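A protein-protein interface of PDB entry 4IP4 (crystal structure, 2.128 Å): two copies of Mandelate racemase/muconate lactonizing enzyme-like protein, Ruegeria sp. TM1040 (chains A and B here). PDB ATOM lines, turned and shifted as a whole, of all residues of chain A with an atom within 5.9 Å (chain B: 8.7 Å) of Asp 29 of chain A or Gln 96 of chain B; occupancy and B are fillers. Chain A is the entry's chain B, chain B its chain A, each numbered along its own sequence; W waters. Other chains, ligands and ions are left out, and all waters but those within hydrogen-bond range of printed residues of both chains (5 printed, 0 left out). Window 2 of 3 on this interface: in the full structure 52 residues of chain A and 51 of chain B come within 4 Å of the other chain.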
ATOM      1  N   SER A  17      10.637 -13.534 -16.763  1.00  0.00           N
ATOM      2  CA  SER A  17       9.677 -12.802 -17.595  1.00  0.00           C
ATOM      3  C   SER A  17       8.982 -13.683 -18.639  1.00  0.00           C
ATOM      4  O   SER A  17       7.900 -13.344 -19.117  1.00  0.00           O
ATOM      5  CB  SER A  17      10.326 -11.587 -18.270  1.00  0.00           C
ATOM      6  OG  SER A  17      11.479 -11.954 -19.003  1.00  0.00           O
ATOM      7  N   LEU A  20       5.961 -14.398 -17.151  1.00  0.00           N
ATOM      8  CA  LEU A  20       5.492 -13.258 -16.364  1.00  0.00           C
ATOM      9  C   LEU A  20       5.367 -13.571 -14.868  1.00  0.00           C
ATOM     10  O   LEU A  20       4.558 -12.964 -14.162  1.00  0.00           O
ATOM     11  CB  LEU A  20       4.178 -12.712 -16.932  1.00  0.00           C
ATOM     12  CG  LEU A  20       4.336 -12.089 -18.325  1.00  0.00           C
ATOM     13  CD1 LEU A  20       3.007 -11.579 -18.878  1.00  0.00           C
ATOM     14  CD2 LEU A  20       5.377 -10.970 -18.280  1.00  0.00           C
ATOM     15  N   SER A  23       5.375 -10.692 -12.197  1.00  0.00           N
ATOM     16  CA  SER A  23       4.769  -9.499 -12.805  1.00  0.00           C
ATOM     17  C   SER A  23       3.836  -8.775 -11.831  1.00  0.00           C
ATOM     18  O   SER A  23       3.105  -9.404 -11.057  1.00  0.00           O
ATOM     19  CB  SER A  23       4.008  -9.860 -14.082  1.00  0.00           C
ATOM     20  OG  SER A  23       2.950 -10.760 -13.797  1.00  0.00           O
ATOM     21  N   ASP A  24       3.891  -7.452 -11.848  1.00  0.00           N
ATOM     22  CA  ASP A  24       3.047  -6.645 -10.969  1.00  0.00           C
ATOM     23  C   ASP A  24       2.758  -5.295 -11.629  1.00  0.00           C
ATOM     24  O   ASP A  24       3.167  -5.062 -12.778  1.00  0.00           O
ATOM     25  CB  ASP A  24       3.670  -6.495  -9.560  1.00  0.00           C
ATOM     26  CG  ASP A  24       4.998  -5.737  -9.564  1.00  0.00           C
ATOM     27  OD1 ASP A  24       5.042  -4.608 -10.102  1.00  0.00           O
ATOM     28  OD2 ASP A  24       6.002  -6.267  -9.013  1.00  0.00           O
ATOM     29  N   ASN A  27       6.243  -3.449 -12.099  1.00  0.00           N
ATOM     30  CA  ASN A  27       7.249  -4.243 -12.796  1.00  0.00           C
ATOM     31  C   ASN A  27       6.591  -5.307 -13.658  1.00  0.00           C
ATOM     32  O   ASN A  27       6.262  -6.384 -13.159  1.00  0.00           O
ATOM     33  CB  ASN A  27       8.168  -4.911 -11.768  1.00  0.00           C
ATOM     34  CG  ASN A  27       8.568  -3.965 -10.671  1.00  0.00           C
ATOM     35  OD1 ASN A  27       9.259  -2.976 -10.924  1.00  0.00           O
ATOM     36  ND2 ASN A  27       8.113  -4.235  -9.445  1.00  0.00           N
ATOM     37  N   PRO A  28       6.390  -5.006 -14.952  1.00  0.00           N
ATOM     38  CA  PRO A  28       5.590  -5.862 -15.841  1.00  0.00           C
ATOM     39  C   PRO A  28       6.288  -7.168 -16.207  1.00  0.00           C
ATOM     40  O   PRO A  28       5.621  -8.157 -16.502  1.00  0.00           O
ATOM     41  CB  PRO A  28       5.430  -5.014 -17.121  1.00  0.00           C
ATOM     42  CG  PRO A  28       5.947  -3.658 -16.790  1.00  0.00           C
ATOM     43  CD  PRO A  28       6.908  -3.816 -15.651  1.00  0.00           C
ATOM     44  N   ASP A  29       7.615  -7.152 -16.220  1.00  0.00           N
ATOM     45  CA  ASP A  29       8.374  -8.275 -16.756  1.00  0.00           C
ATOM     46  C   ASP A  29       9.723  -8.444 -16.073  1.00  0.00           C
ATOM     47  O   ASP A  29      10.751  -8.502 -16.750  1.00  0.00           O
ATOM     48  CB  ASP A  29       8.587  -8.079 -18.262  1.00  0.00           C
ATOM     49  CG  ASP A  29       9.304  -6.767 -18.590  1.00  0.00           C
ATOM     50  OD1 ASP A  29       9.360  -5.870 -17.718  1.00  0.00           O
ATOM     51  OD2 ASP A  29       9.819  -6.634 -19.719  1.00  0.00           O
ATOM     52  N   PRO A  30       9.728  -8.539 -14.732  1.00  0.00           N
ATOM     53  CA  PRO A  30      11.007  -8.688 -14.028  1.00  0.00           C
ATOM     54  C   PRO A  30      11.757  -9.948 -14.441  1.00  0.00           C
ATOM     55  O   PRO A  30      11.144 -10.984 -14.708  1.00  0.00           O
ATOM     56  CB  PRO A  30      10.587  -8.798 -12.554  1.00  0.00           C
ATOM     57  CG  PRO A  30       9.197  -9.341 -12.603  1.00  0.00           C
ATOM     58  CD  PRO A  30       8.578  -8.691 -13.819  1.00  0.00           C
ATOM     59  N   ASP A  31      13.078  -9.833 -14.526  1.00  0.00           N
ATOM     60  CA  ASP A  31      13.958 -10.984 -14.667  1.00  0.00           C
ATOM     61  C   ASP A  31      14.709 -11.129 -13.354  1.00  0.00           C
ATOM     62  O   ASP A  31      15.719 -10.448 -13.125  1.00  0.00           O
ATOM     63  CB  ASP A  31      14.933 -10.780 -15.823  1.00  0.00           C
ATOM     64  CG  ASP A  31      14.261 -10.898 -17.169  1.00  0.00           C
ATOM     65  OD1 ASP A  31      13.445 -11.833 -17.351  1.00  0.00           O
ATOM     66  OD2 ASP A  31      14.540 -10.048 -18.038  1.00  0.00           O
ATOM     67  N   THR A  53      17.775  -8.197  -7.474  1.00  0.00           N
ATOM     68  CA  THR A  53      17.286  -7.179  -8.398  1.00  0.00           C
ATOM     69  C   THR A  53      16.419  -7.887  -9.430  1.00  0.00           C
ATOM     70  O   THR A  53      16.274  -9.110  -9.381  1.00  0.00           O
ATOM     71  CB  THR A  53      18.431  -6.397  -9.099  1.00  0.00           C
ATOM     72  OG1 THR A  53      19.074  -7.226 -10.074  1.00  0.00           O
ATOM     73  CG2 THR A  53      19.471  -5.906  -8.084  1.00  0.00           C
ATOM     74  N   ILE A  54      15.829  -7.133 -10.353  1.00  0.00           N
ATOM     75  CA  ILE A  54      14.955  -7.738 -11.352  1.00  0.00           C
ATOM     76  C   ILE A  54      15.448  -7.577 -12.792  1.00  0.00           C
ATOM     77  O   ILE A  54      14.650  -7.502 -13.726  1.00  0.00           O
ATOM     78  CB  ILE A  54      13.504  -7.235 -11.230  1.00  0.00           C
ATOM     79  CG1 ILE A  54      13.441  -5.704 -11.283  1.00  0.00           C
ATOM     80  CG2 ILE A  54      12.877  -7.743  -9.938  1.00  0.00           C
ATOM     81  CD1 ILE A  54      12.015  -5.159 -11.348  1.00  0.00           C
ATOM     82  N   GLY A  55      16.765  -7.550 -12.968  1.00  0.00           N
ATOM     83  CA  GLY A  55      17.348  -7.579 -14.297  1.00  0.00           C
ATOM     84  C   GLY A  55      18.354  -6.470 -14.544  1.00  0.00           C
ATOM     85  O   GLY A  55      19.426  -6.434 -13.928  1.00  0.00           O
ATOM     86  N   ARG A  56      18.017  -5.574 -15.463  1.00  0.00           N
ATOM     87  CA  ARG A  56      18.889  -4.443 -15.768  1.00  0.00           C
ATOM     88  C   ARG A  56      19.193  -3.686 -14.484  1.00  0.00           C
ATOM     89  O   ARG A  56      18.308  -3.496 -13.643  1.00  0.00           O
ATOM     90  CB  ARG A  56      18.237  -3.522 -16.799  1.00  0.00           C
ATOM     91  CG  ARG A  56      17.993  -4.188 -18.155  1.00  0.00           C
ATOM     92  CD  ARG A  56      17.262  -3.251 -19.105  1.00  0.00           C
ATOM     93  NE  ARG A  56      15.945  -2.902 -18.584  1.00  0.00           N
ATOM     94  CZ  ARG A  56      14.843  -3.611 -18.809  1.00  0.00           C
ATOM     95  NH1 ARG A  56      14.902  -4.715 -19.548  1.00  0.00           N
ATOM     96  NH2 ARG A  56      13.683  -3.222 -18.293  1.00  0.00           N
ATOM     97  N   GLY A  57      20.447  -3.275 -14.322  1.00  0.00           N
ATOM     98  CA  GLY A  57      20.866  -2.626 -13.091  1.00  0.00           C
ATOM     99  C   GLY A  57      21.588  -3.567 -12.139  1.00  0.00           C
ATOM    100  O   GLY A  57      22.244  -3.110 -11.204  1.00  0.00           O
ATOM    101  N   ALA B  67      24.064   2.522 -17.821  1.00  0.00           N
ATOM    102  CA  ALA B  67      22.781   1.829 -17.819  1.00  0.00           C
ATOM    103  C   ALA B  67      21.654   2.725 -18.352  1.00  0.00           C
ATOM    104  O   ALA B  67      20.846   2.283 -19.160  1.00  0.00           O
ATOM    105  CB  ALA B  67      22.451   1.323 -16.413  1.00  0.00           C
ATOM    106  N   LEU B  71      18.337   4.156 -22.323  1.00  0.00           N
ATOM    107  CA  LEU B  71      17.045   4.844 -22.376  1.00  0.00           C
ATOM    108  C   LEU B  71      17.097   6.134 -23.188  1.00  0.00           C
ATOM    109  O   LEU B  71      16.062   6.652 -23.617  1.00  0.00           O
ATOM    110  CB  LEU B  71      16.544   5.158 -20.964  1.00  0.00           C
ATOM    111  CG  LEU B  71      16.307   3.951 -20.049  1.00  0.00           C
ATOM    112  CD1 LEU B  71      15.884   4.407 -18.671  1.00  0.00           C
ATOM    113  CD2 LEU B  71      15.265   2.991 -20.636  1.00  0.00           C
ATOM    114  N   THR B  92      13.595   7.751 -15.743  1.00  0.00           N
ATOM    115  CA  THR B  92      13.536   7.193 -14.391  1.00  0.00           C
ATOM    116  C   THR B  92      12.497   6.087 -14.299  1.00  0.00           C
ATOM    117  O   THR B  92      12.202   5.614 -13.203  1.00  0.00           O
ATOM    118  CB  THR B  92      13.166   8.265 -13.343  1.00  0.00           C
ATOM    119  OG1 THR B  92      11.833   8.746 -13.593  1.00  0.00           O
ATOM    120  CG2 THR B  92      14.145   9.428 -13.396  1.00  0.00           C
ATOM    121  N   GLY B  93      11.942   5.683 -15.442  1.00  0.00           N
ATOM    122  CA  GLY B  93      10.807   4.762 -15.461  1.00  0.00           C
ATOM    123  C   GLY B  93      11.039   3.320 -15.884  1.00  0.00           C
ATOM    124  O   GLY B  93      10.085   2.536 -15.978  1.00  0.00           O
ATOM    125  N   ASP B  94      12.286   2.956 -16.163  1.00  0.00           N
ATOM    126  CA  ASP B  94      12.607   1.551 -16.396  1.00  0.00           C
ATOM    127  C   ASP B  94      12.459   0.843 -15.054  1.00  0.00           C
ATOM    128  O   ASP B  94      13.275   1.050 -14.153  1.00  0.00           O
ATOM    129  CB  ASP B  94      14.035   1.414 -16.924  1.00  0.00           C
ATOM    130  CG  ASP B  94      14.436  -0.027 -17.205  1.00  0.00           C
ATOM    131  OD1 ASP B  94      13.880  -0.962 -16.595  1.00  0.00           O
ATOM    132  OD2 ASP B  94      15.336  -0.227 -18.043  1.00  0.00           O
ATOM    133  N   SER B  95      11.430   0.004 -14.930  1.00  0.00           N
ATOM    134  CA  SER B  95      11.102  -0.634 -13.651  1.00  0.00           C
ATOM    135  C   SER B  95      12.273  -1.417 -13.063  1.00  0.00           C
ATOM    136  O   SER B  95      12.436  -1.481 -11.846  1.00  0.00           O
ATOM    137  CB  SER B  95       9.881  -1.548 -13.796  1.00  0.00           C
ATOM    138  OG  SER B  95      10.134  -2.595 -14.714  1.00  0.00           O
ATOM    139  N   GLN B  96      13.093  -1.998 -13.930  1.00  0.00           N
ATOM    140  CA  GLN B  96      14.255  -2.753 -13.479  1.00  0.00           C
ATOM    141  C   GLN B  96      15.355  -1.835 -12.919  1.00  0.00           C
ATOM    142  O   GLN B  96      15.948  -2.123 -11.869  1.00  0.00           O
ATOM    143  CB  GLN B  96      14.771  -3.668 -14.598  1.00  0.00           C
ATOM    144  CG  GLN B  96      13.727  -4.714 -15.030  1.00  0.00           C
ATOM    145  CD  GLN B  96      14.213  -5.653 -16.118  1.00  0.00           C
ATOM    146  OE1 GLN B  96      15.407  -5.721 -16.418  1.00  0.00           O
ATOM    147  NE2 GLN B  96      13.281  -6.383 -16.720  1.00  0.00           N
ATOM    148  N   LEU B  97      15.612  -0.722 -13.601  1.00  0.00           N
ATOM    149  CA  LEU B  97      16.538   0.272 -13.062  1.00  0.00           C
ATOM    150  C   LEU B  97      15.960   0.948 -11.802  1.00  0.00           C
ATOM    151  O   LEU B  97      16.709   1.348 -10.905  1.00  0.00           O
ATOM    152  CB  LEU B  97      16.946   1.295 -14.132  1.00  0.00           C
ATOM    153  CG  LEU B  97      17.750   0.750 -15.324  1.00  0.00           C
ATOM    154  CD1 LEU B  97      18.095   1.872 -16.305  1.00  0.00           C
ATOM    155  CD2 LEU B  97      19.026   0.025 -14.880  1.00  0.00           C
ATOM    156  N   ARG B  98      14.636   1.048 -11.727  1.00  0.00           N
ATOM    157  CA  ARG B  98      13.967   1.554 -10.519  1.00  0.00           C
ATOM    158  C   ARG B  98      14.248   0.698  -9.302  1.00  0.00           C
ATOM    159  O   ARG B  98      14.395   1.220  -8.197  1.00  0.00           O
ATOM    160  CB  ARG B  98      12.453   1.643 -10.714  1.00  0.00           C
ATOM    161  CG  ARG B  98      12.015   2.839 -11.560  1.00  0.00           C
ATOM    162  CD  ARG B  98      10.494   2.971 -11.591  1.00  0.00           C
ATOM    163  NE  ARG B  98       9.939   3.540 -10.360  1.00  0.00           N
ATOM    164  CZ  ARG B  98      10.021   4.828 -10.033  1.00  0.00           C
ATOM    165  NH1 ARG B  98      10.662   5.680 -10.830  1.00  0.00           N
ATOM    166  NH2 ARG B  98       9.471   5.272  -8.908  1.00  0.00           N
ATOM    167  N   TRP B  99      14.318  -0.617  -9.502  1.00  0.00           N
ATOM    168  CA  TRP B  99      14.626  -1.526  -8.400  1.00  0.00           C
ATOM    169  C   TRP B  99      15.920  -1.136  -7.663  1.00  0.00           C
ATOM    170  O   TRP B  99      16.036  -1.331  -6.458  1.00  0.00           O
ATOM    171  CB  TRP B  99      14.730  -2.971  -8.894  1.00  0.00           C
ATOM    172  CG  TRP B  99      14.544  -3.937  -7.794  1.00  0.00           C
ATOM    173  CD1 TRP B  99      15.511  -4.434  -6.970  1.00  0.00           C
ATOM    174  CD2 TRP B  99      13.308  -4.507  -7.351  1.00  0.00           C
ATOM    175  NE1 TRP B  99      14.960  -5.294  -6.058  1.00  0.00           N
ATOM    176  CE2 TRP B  99      13.608  -5.359  -6.268  1.00  0.00           C
ATOM    177  CE3 TRP B  99      11.982  -4.402  -7.782  1.00  0.00           C
ATOM    178  CZ2 TRP B  99      12.631  -6.082  -5.594  1.00  0.00           C
ATOM    179  CZ3 TRP B  99      11.008  -5.129  -7.112  1.00  0.00           C
ATOM    180  CH2 TRP B  99      11.337  -5.959  -6.034  1.00  0.00           C
ATOM    181  N   ILE B 100      16.877  -0.581  -8.401  1.00  0.00           N
ATOM    182  CA  ILE B 100      18.182  -0.197  -7.853  1.00  0.00           C
ATOM    183  C   ILE B 100      18.068   1.079  -7.007  1.00  0.00           C
ATOM    184  O   ILE B 100      18.973   1.428  -6.253  1.00  0.00           O
ATOM    185  CB  ILE B 100      19.190   0.012  -9.016  1.00  0.00           C
ATOM    186  CG1 ILE B 100      19.107  -1.166  -9.991  1.00  0.00           C
ATOM    187  CG2 ILE B 100      20.615   0.183  -8.516  1.00  0.00           C
ATOM    188  CD1 ILE B 100      19.303  -2.530  -9.328  1.00  0.00           C
ATOM    189  N   GLY B 101      16.944   1.780  -7.156  1.00  0.00           N
ATOM    190  CA  GLY B 101      16.638   2.960  -6.367  1.00  0.00           C
ATOM    191  C   GLY B 101      15.471   2.653  -5.434  1.00  0.00           C
ATOM    192  O   GLY B 101      15.657   1.962  -4.433  1.00  0.00           O
ATOM    193  N   PRO B 102      14.262   3.164  -5.754  1.00  0.00           N
ATOM    194  CA  PRO B 102      13.974   4.055  -6.890  1.00  0.00           C
ATOM    195  C   PRO B 102      14.247   5.515  -6.554  1.00  0.00           C
ATOM    196  O   PRO B 102      13.984   5.940  -5.424  1.00  0.00           O
ATOM    197  CB  PRO B 102      12.461   3.864  -7.129  1.00  0.00           C
ATOM    198  CG  PRO B 102      12.032   2.705  -6.180  1.00  0.00           C
ATOM    199  CD  PRO B 102      13.028   2.756  -5.062  1.00  0.00           C
ATOM    200  N   ILE B 107      21.730   5.243  -8.981  1.00  0.00           N
ATOM    201  CA  ILE B 107      20.905   5.334 -10.179  1.00  0.00           C
ATOM    202  C   ILE B 107      20.356   6.753 -10.340  1.00  0.00           C
ATOM    203  O   ILE B 107      20.203   7.240 -11.460  1.00  0.00           O
ATOM    204  CB  ILE B 107      19.755   4.277 -10.181  1.00  0.00           C
ATOM    205  CG1 ILE B 107      19.161   4.127 -11.583  1.00  0.00           C
ATOM    206  CG2 ILE B 107      18.674   4.630  -9.156  1.00  0.00           C
ATOM    207  CD1 ILE B 107      20.161   3.654 -12.644  1.00  0.00           C
HETATM  208  O   HOH W   1      12.332  -8.520 -18.763  1.00  0.00           O
HETATM  209  O   HOH W   2      16.697  -4.571 -11.378  1.00  0.00           O
HETATM  210  O   HOH W   3      16.135  -8.020 -17.875  1.00  0.00           O
HETATM  211  O   HOH W   4      10.689  -1.089  -9.571  1.00  0.00           O
HETATM  212  O   HOH W   5      10.074  -5.460 -15.072  1.00  0.00           O
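The backbone NH (N) of Gln 96 of chain B sits at hydrogen-bond distance from the side-chain carboxylate (OD1) of Asp 94 of chain B, at 3.0 Å.
OD1 of Asp 94 of chain B sits at hydrogen-bond distance from N of Leu 97 of chain B.
The backbone NH (N) of Asn 27 of chain A is in hydrogen-bond range of the side-chain carboxylate (OD1) of Asp 24 of chain A, 2.6 Å away.
O of Ile 54 of chain A sits at hydrogen-bond distance from N of Asp 31 of chain A.
The backbone NH of Gly 55 of chain A lies within hydrogen-bond range of the backbone carbonyl oxygen of Asp 31 of chain A (3.1 Å).
Asn 27 of chain A touches Ser 95 of chain B.
CZ3 of Trp 99 of chain B touches ND2 of Asn 27 of chain A, at 3.8 Å.
Ser 95 of chain B touches Pro 28 of chain A.
Trp 99 of chain B touches Thr 53 of chain A (CD1 to CA, 3.6 Å).
Thr 53 of chain A touches Ile 100 of chain B (CG2 to CD1, 3.6 Å).
Ile 54 of chain A touches Ser 95 of chain B (CD1 to O, 3.7 Å).
Ile 54 of chain A touches Trp 99 of chain B (CD1 to CE3, 3.6 Å).
Arg 56 of chain A touches Leu 97 of chain B.
N of Gly 57 of chain A touches CD2 of Leu 97 of chain B, at 3.6 Å.
Gly 57 of chain A touches Ile 100 of chain B.
No position is printed for both chains.
Of the 15 pairs that touch across the chains among the printed residues, none has its exchanged pair printed and touching as well.
NE of Arg 56 of chain A lies within salt-bridge range of OD2 of Asp 94 of chain B, at 2.8 Å.
The side-chain amide nitrogen (NE2) of Gln 96 of chain B is in hydrogen-bond range of the backbone carbonyl oxygen (O) of Asp 29 of chain A (3.3 Å).
O of Ile 54 of chain A lies close to OE1 of Gln 96 of chain B (3.3 Å).
OE1 of Gln 96 of chain B lies within hydrogen-bond range of N of Arg 56 of chain A (2.8 Å).
Asp 29 of chain A touches just one residue of chain B: Gln 96 (3.3 Å).
Gln 96 of chain B touches just these residues of chain A: Asp 29, Ile 54, Gly 55 and Arg 56.
Pro 28 of chain A touches just one residue of chain B: Ser 95.
Arg 56 of chain A touches three residues of chain B.
Printed residues of chain A within 4 Å of Ile 100 of chain B: Thr 53 (3.6 Å) and Gly 57 (3.5 Å).
Printed residues of chain B within 4 Å of Thr 53 of chain A: Trp 99 (3.6 Å) and Ile 100 (3.6 Å).
Of the printed residues of chain B, Ile 54 of chain A touches Ser 95, Gln 96 and Trp 99.
The nearest residue of chain B that does not touch Asp 29 of chain A is Ser 95 of chain B (4.5 Å).
The nearest residue of chain A that does not touch Gln 96 of chain B is Asp 31 of chain A (4.1 Å).
The nearest printed residue of chain B that does not touch Asn 27 of chain A is Gln 96 of chain B (5.0 Å).
Water W1 lies within hydrogen-bond range of O of Asp 29 of chain A (2.6 Å), OD2 of Asp 31 of chain A (2.8 Å) and NE2 of Gln 96 of chain B (3.1 Å).
Water W3 bridges the side-chain carboxylate of Asp 31 of chain A (2.6 Å) and the side-chain amide oxygen of Gln 96 of chain B (2.8 Å).
Water W2 lies within hydrogen-bond range of O of Gln 96 of chain B, N of Ile 54 of chain A, O of Arg 56 of chain A and N of Gly 55 of chain A.
Water W4 bridges OD1 of Asn 27 of chain A (2.7 Å) and O of Ser 95 of chain B (2.9 Å).
Water W5 bridges OD1 of Asp 29 of chain A and OG of Ser 95 of chain B.
Of the 14 printed residues of chain B, 6 touch a printed residue of chain A.
Hydrophobic or aromatic side chains of chain B that line the printed part of chain A: Leu 97, Trp 99 and Ile 100.
Printed residues of chain A that touch a printed residue of chain B: Asn 27, Pro 28, Asp 29, Thr 53, Ile 54, Gly 55, Arg 56 and Gly 57.
Among the printed residues, 15 pairs touch across the chains.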
